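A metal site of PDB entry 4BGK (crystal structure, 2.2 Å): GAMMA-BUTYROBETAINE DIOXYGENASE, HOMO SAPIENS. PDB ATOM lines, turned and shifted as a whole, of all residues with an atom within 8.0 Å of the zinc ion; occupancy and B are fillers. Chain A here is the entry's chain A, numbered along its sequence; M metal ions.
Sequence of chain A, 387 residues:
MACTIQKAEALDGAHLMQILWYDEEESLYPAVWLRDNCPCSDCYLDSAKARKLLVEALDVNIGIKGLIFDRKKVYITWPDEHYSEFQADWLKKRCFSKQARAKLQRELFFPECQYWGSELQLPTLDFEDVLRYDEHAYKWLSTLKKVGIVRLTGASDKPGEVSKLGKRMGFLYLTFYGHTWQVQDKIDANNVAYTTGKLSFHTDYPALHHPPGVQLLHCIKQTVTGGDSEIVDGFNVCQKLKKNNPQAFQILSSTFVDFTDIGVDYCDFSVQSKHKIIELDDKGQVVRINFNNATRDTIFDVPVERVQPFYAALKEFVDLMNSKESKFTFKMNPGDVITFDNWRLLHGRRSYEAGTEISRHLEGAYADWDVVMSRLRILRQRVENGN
The side-chain hydroxyl (OG) of Ser 84 lies close to the side-chain sulfur (SG) of Cys 38, at 3.0 Å. The side-chain sulfur (SG) of Cys 40 lies close to the backbone NH (N) of Asp 42 (3.4 Å). SG of Cys 43 lies close to NH1 of Arg 35 (3.3 Å). The backbone NH (N) of Leu 53 lies within hydrogen-bond range of the backbone carbonyl oxygen (O) of Cys 43 (3.2 Å).
Of the 18 residues printed, 4 come within 4 Å of the zinc ion. The nearest printed residue that does not touch the zinc ion is Arg 35 (4.1 Å).
The zinc ion is bound by a ring nitrogen (NE2) of His 82 (2.1 Å), the side-chain sulfur of Cys 38 (2.3 Å), the side-chain sulfur of Cys 40 (2.3 Å) and the side-chain sulfur of Cys 43 (2.3 Å).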
ATOM      1  N   LEU A  34       6.479  18.256  -9.876  1.00  0.00           N
ATOM      2  CA  LEU A  34       7.013  19.160  -8.873  1.00  0.00           C
ATOM      3  C   LEU A  34       5.958  19.469  -7.844  1.00  0.00           C
ATOM      4  O   LEU A  34       6.208  19.351  -6.657  1.00  0.00           O
ATOM      5  CB  LEU A  34       7.520  20.455  -9.505  1.00  0.00           C
ATOM      6  CG  LEU A  34       8.794  20.298 -10.349  1.00  0.00           C
ATOM      7  CD1 LEU A  34       8.982  21.531 -11.207  1.00  0.00           C
ATOM      8  CD2 LEU A  34      10.012  20.051  -9.470  1.00  0.00           C
ATOM      9  N   ARG A  35       4.777  19.857  -8.279  1.00  0.00           N
ATOM     10  CA  ARG A  35       3.708  20.162  -7.335  1.00  0.00           C
ATOM     11  C   ARG A  35       3.335  18.957  -6.480  1.00  0.00           C
ATOM     12  O   ARG A  35       3.162  19.077  -5.241  1.00  0.00           O
ATOM     13  CB  ARG A  35       2.463  20.629  -8.075  1.00  0.00           C
ATOM     14  CG  ARG A  35       1.302  21.024  -7.163  1.00  0.00           C
ATOM     15  CD  ARG A  35       1.650  22.231  -6.293  1.00  0.00           C
ATOM     16  NE  ARG A  35       0.650  22.490  -5.264  1.00  0.00           N
ATOM     17  CZ  ARG A  35       0.594  21.869  -4.090  1.00  0.00           C
ATOM     18  NH1 ARG A  35       1.501  20.950  -3.799  1.00  0.00           N
ATOM     19  NH2 ARG A  35      -0.357  22.175  -3.203  1.00  0.00           N
ATOM     20  N   ASP A  36       3.197  17.810  -7.155  1.00  0.00           N
ATOM     21  CA  ASP A  36       2.921  16.524  -6.495  1.00  0.00           C
ATOM     22  C   ASP A  36       3.922  16.227  -5.386  1.00  0.00           C
ATOM     23  O   ASP A  36       3.562  15.637  -4.379  1.00  0.00           O
ATOM     24  CB  ASP A  36       2.968  15.381  -7.513  1.00  0.00           C
ATOM     25  CG  ASP A  36       2.681  14.036  -6.894  1.00  0.00           C
ATOM     26  OD1 ASP A  36       1.647  13.924  -6.166  1.00  0.00           O
ATOM     27  OD2 ASP A  36       3.467  13.084  -7.148  1.00  0.00           O
ATOM     28  N   ASN A  37       5.157  16.689  -5.580  1.00  0.00           N
ATOM     29  CA  ASN A  37       6.237  16.372  -4.666  1.00  0.00           C
ATOM     30  C   ASN A  37       6.780  17.550  -3.881  1.00  0.00           C
ATOM     31  O   ASN A  37       7.889  17.486  -3.380  1.00  0.00           O
ATOM     32  CB  ASN A  37       7.340  15.633  -5.423  1.00  0.00           C
ATOM     33  CG  ASN A  37       6.910  14.249  -5.827  1.00  0.00           C
ATOM     34  OD1 ASN A  37       6.652  13.428  -4.967  1.00  0.00           O
ATOM     35  ND2 ASN A  37       6.788  14.002  -7.129  1.00  0.00           N
ATOM     36  N   CYS A  38       5.955  18.592  -3.726  1.00  0.00           N
ATOM     37  CA  CYS A  38       6.242  19.672  -2.775  1.00  0.00           C
ATOM     38  C   CYS A  38       6.599  19.096  -1.404  1.00  0.00           C
ATOM     39  O   CYS A  38       5.828  18.322  -0.863  1.00  0.00           O
ATOM     40  CB  CYS A  38       5.022  20.567  -2.598  1.00  0.00           C
ATOM     41  SG  CYS A  38       5.340  21.977  -1.513  1.00  0.00           S
ATOM     42  N   PRO A  39       7.765  19.478  -0.852  1.00  0.00           N
ATOM     43  CA  PRO A  39       8.163  18.974   0.470  1.00  0.00           C
ATOM     44  C   PRO A  39       7.670  19.757   1.696  1.00  0.00           C
ATOM     45  O   PRO A  39       8.057  19.433   2.793  1.00  0.00           O
ATOM     46  CB  PRO A  39       9.706  18.993   0.410  1.00  0.00           C
ATOM     47  CG  PRO A  39      10.032  20.065  -0.592  1.00  0.00           C
ATOM     48  CD  PRO A  39       8.862  20.207  -1.517  1.00  0.00           C
ATOM     49  N   CYS A  40       6.830  20.783   1.510  1.00  0.00           N
ATOM     50  CA  CYS A  40       6.357  21.579   2.616  1.00  0.00           C
ATOM     51  C   CYS A  40       5.504  20.746   3.567  1.00  0.00           C
ATOM     52  O   CYS A  40       5.041  19.637   3.250  1.00  0.00           O
ATOM     53  CB  CYS A  40       5.579  22.836   2.119  1.00  0.00           C
ATOM     54  SG  CYS A  40       3.792  22.653   1.847  1.00  0.00           S
ATOM     55  N   SER A  41       5.302  21.290   4.759  1.00  0.00           N
ATOM     56  CA  SER A  41       4.643  20.559   5.825  1.00  0.00           C
ATOM     57  C   SER A  41       3.169  20.347   5.551  1.00  0.00           C
ATOM     58  O   SER A  41       2.568  19.445   6.133  1.00  0.00           O
ATOM     59  CB  SER A  41       4.902  21.243   7.180  1.00  0.00           C
ATOM     60  OG  SER A  41       4.131  22.420   7.314  1.00  0.00           O
ATOM     61  N   ASP A  42       2.567  21.126   4.626  1.00  0.00           N
ATOM     62  CA  ASP A  42       1.198  20.833   4.189  1.00  0.00           C
ATOM     63  C   ASP A  42       1.130  19.584   3.281  1.00  0.00           C
ATOM     64  O   ASP A  42       0.170  18.797   3.325  1.00  0.00           O
ATOM     65  CB  ASP A  42       0.609  22.032   3.428  1.00  0.00           C
ATOM     66  CG  ASP A  42       0.280  23.209   4.335  1.00  0.00           C
ATOM     67  OD1 ASP A  42       0.451  23.108   5.554  1.00  0.00           O
ATOM     68  OD2 ASP A  42      -0.174  24.230   3.832  1.00  0.00           O
ATOM     69  N   CYS A  43       2.163  19.438   2.458  1.00  0.00           N
ATOM     70  CA  CYS A  43       2.163  18.478   1.388  1.00  0.00           C
ATOM     71  C   CYS A  43       2.855  17.182   1.743  1.00  0.00           C
ATOM     72  O   CYS A  43       2.616  16.154   1.117  1.00  0.00           O
ATOM     73  CB  CYS A  43       2.829  19.066   0.157  1.00  0.00           C
ATOM     74  SG  CYS A  43       1.898  20.435  -0.553  1.00  0.00           S
ATOM     75  N   TYR A  44       3.713  17.257   2.752  1.00  0.00           N
ATOM     76  CA  TYR A  44       4.636  16.190   3.048  1.00  0.00           C
ATOM     77  C   TYR A  44       4.810  16.026   4.546  1.00  0.00           C
ATOM     78  O   TYR A  44       5.114  17.011   5.235  1.00  0.00           O
ATOM     79  CB  TYR A  44       5.978  16.504   2.420  1.00  0.00           C
ATOM     80  CG  TYR A  44       6.897  15.312   2.355  1.00  0.00           C
ATOM     81  CD1 TYR A  44       6.747  14.361   1.370  1.00  0.00           C
ATOM     82  CD2 TYR A  44       7.906  15.138   3.285  1.00  0.00           C
ATOM     83  CE1 TYR A  44       7.571  13.266   1.297  1.00  0.00           C
ATOM     84  CE2 TYR A  44       8.753  14.057   3.218  1.00  0.00           C
ATOM     85  CZ  TYR A  44       8.583  13.120   2.220  1.00  0.00           C
ATOM     86  OH  TYR A  44       9.417  12.008   2.143  1.00  0.00           O
ATOM     87  N   LEU A  53      -0.303  15.141   0.424  1.00  0.00           N
ATOM     88  CA  LEU A  53      -1.049  15.705  -0.670  1.00  0.00           C
ATOM     89  C   LEU A  53      -1.924  14.650  -1.319  1.00  0.00           C
ATOM     90  O   LEU A  53      -1.478  13.530  -1.578  1.00  0.00           O
ATOM     91  CB  LEU A  53      -0.085  16.290  -1.713  1.00  0.00           C
ATOM     92  CG  LEU A  53      -0.645  17.166  -2.820  1.00  0.00           C
ATOM     93  CD1 LEU A  53      -1.243  18.466  -2.316  1.00  0.00           C
ATOM     94  CD2 LEU A  53       0.484  17.404  -3.825  1.00  0.00           C
ATOM     95  N   TRP A  78       3.021  28.700  -7.323  1.00  0.00           N
ATOM     96  CA  TRP A  78       1.989  28.052  -8.117  1.00  0.00           C
ATOM     97  C   TRP A  78       0.783  28.996  -8.332  1.00  0.00           C
ATOM     98  O   TRP A  78       0.644  29.997  -7.633  1.00  0.00           O
ATOM     99  CB  TRP A  78       1.553  26.778  -7.424  1.00  0.00           C
ATOM    100  CG  TRP A  78       2.668  25.821  -7.248  1.00  0.00           C
ATOM    101  CD1 TRP A  78       3.319  25.509  -6.095  1.00  0.00           C
ATOM    102  CD2 TRP A  78       3.280  25.050  -8.275  1.00  0.00           C
ATOM    103  NE1 TRP A  78       4.298  24.582  -6.337  1.00  0.00           N
ATOM    104  CE2 TRP A  78       4.298  24.284  -7.666  1.00  0.00           C
ATOM    105  CE3 TRP A  78       3.080  24.947  -9.651  1.00  0.00           C
ATOM    106  CZ2 TRP A  78       5.104  23.421  -8.381  1.00  0.00           C
ATOM    107  CZ3 TRP A  78       3.890  24.063 -10.364  1.00  0.00           C
ATOM    108  CH2 TRP A  78       4.890  23.318  -9.737  1.00  0.00           C
ATOM    109  N   HIS A  82       0.121  28.589  -3.714  1.00  0.00           N
ATOM    110  CA  HIS A  82       0.931  27.660  -2.943  1.00  0.00           C
ATOM    111  C   HIS A  82       2.413  27.897  -3.276  1.00  0.00           C
ATOM    112  O   HIS A  82       2.744  28.366  -4.373  1.00  0.00           O
ATOM    113  CB  HIS A  82       0.522  26.207  -3.230  1.00  0.00           C
ATOM    114  CG  HIS A  82       1.102  25.227  -2.268  1.00  0.00           C
ATOM    115  ND1 HIS A  82       0.558  24.969  -1.038  1.00  0.00           N
ATOM    116  CD2 HIS A  82       2.176  24.407  -2.385  1.00  0.00           C
ATOM    117  CE1 HIS A  82       1.295  24.070  -0.417  1.00  0.00           C
ATOM    118  NE2 HIS A  82       2.259  23.696  -1.217  1.00  0.00           N
ATOM    119  N   TYR A  83       3.305  27.567  -2.355  1.00  0.00           N
ATOM    120  CA  TYR A  83       4.718  27.887  -2.534  1.00  0.00           C
ATOM    121  C   TYR A  83       5.577  26.663  -2.254  1.00  0.00           C
ATOM    122  O   TYR A  83       5.284  25.917  -1.340  1.00  0.00           O
ATOM    123  CB  TYR A  83       5.091  29.049  -1.600  1.00  0.00           C
ATOM    124  CG  TYR A  83       6.549  29.308  -1.501  1.00  0.00           C
ATOM    125  CD1 TYR A  83       7.263  29.837  -2.586  1.00  0.00           C
ATOM    126  CD2 TYR A  83       7.255  29.003  -0.324  1.00  0.00           C
ATOM    127  CE1 TYR A  83       8.637  30.068  -2.492  1.00  0.00           C
ATOM    128  CE2 TYR A  83       8.623  29.218  -0.235  1.00  0.00           C
ATOM    129  CZ  TYR A  83       9.309  29.766  -1.319  1.00  0.00           C
ATOM    130  OH  TYR A  83      10.677  29.992  -1.220  1.00  0.00           O
ATOM    131  N   SER A  84       6.603  26.439  -3.070  1.00  0.00           N
ATOM    132  CA  SER A  84       7.439  25.250  -2.923  1.00  0.00           C
ATOM    133  C   SER A  84       8.933  25.561  -3.101  1.00  0.00           C
ATOM    134  O   SER A  84       9.300  26.365  -3.951  1.00  0.00           O
ATOM    135  CB  SER A  84       7.043  24.163  -3.951  1.00  0.00           C
ATOM    136  OG  SER A  84       5.666  23.820  -3.906  1.00  0.00           O
ATOM    137  N   GLU A  85       9.765  24.885  -2.329  1.00  0.00           N
ATOM    138  CA  GLU A  85      11.216  24.913  -2.489  1.00  0.00           C
ATOM    139  C   GLU A  85      11.759  23.529  -2.735  1.00  0.00           C
ATOM    140  O   GLU A  85      11.351  22.570  -2.091  1.00  0.00           O
ATOM    141  CB  GLU A  85      11.881  25.464  -1.219  1.00  0.00           C
ATOM    142  CG  GLU A  85      11.321  26.817  -0.806  1.00  0.00           C
ATOM    143  CD  GLU A  85      12.093  27.475   0.324  1.00  0.00           C
ATOM    144  OE1 GLU A  85      12.948  26.805   0.953  1.00  0.00           O
ATOM    145  OE2 GLU A  85      11.849  28.667   0.558  1.00  0.00           O
ATOM    146  N   PHE A  86      12.693  23.426  -3.671  1.00  0.00           N
ATOM    147  CA  PHE A  86      13.329  22.168  -4.016  1.00  0.00           C
ATOM    148  C   PHE A  86      14.822  22.331  -3.991  1.00  0.00           C
ATOM    149  O   PHE A  86      15.347  23.306  -4.519  1.00  0.00           O
ATOM    150  CB  PHE A  86      12.897  21.729  -5.408  1.00  0.00           C
ATOM    151  CG  PHE A  86      11.400  21.550  -5.557  1.00  0.00           C
ATOM    152  CD1 PHE A  86      10.802  20.352  -5.229  1.00  0.00           C
ATOM    153  CD2 PHE A  86      10.618  22.585  -6.035  1.00  0.00           C
ATOM    154  CE1 PHE A  86       9.433  20.191  -5.362  1.00  0.00           C
ATOM    155  CE2 PHE A  86       9.250  22.438  -6.172  1.00  0.00           C
ATOM    156  CZ  PHE A  86       8.656  21.228  -5.831  1.00  0.00           C
HETATM  157 ZN    ZN M   1       3.404  22.170  -0.359  1.00  0.00          ZN
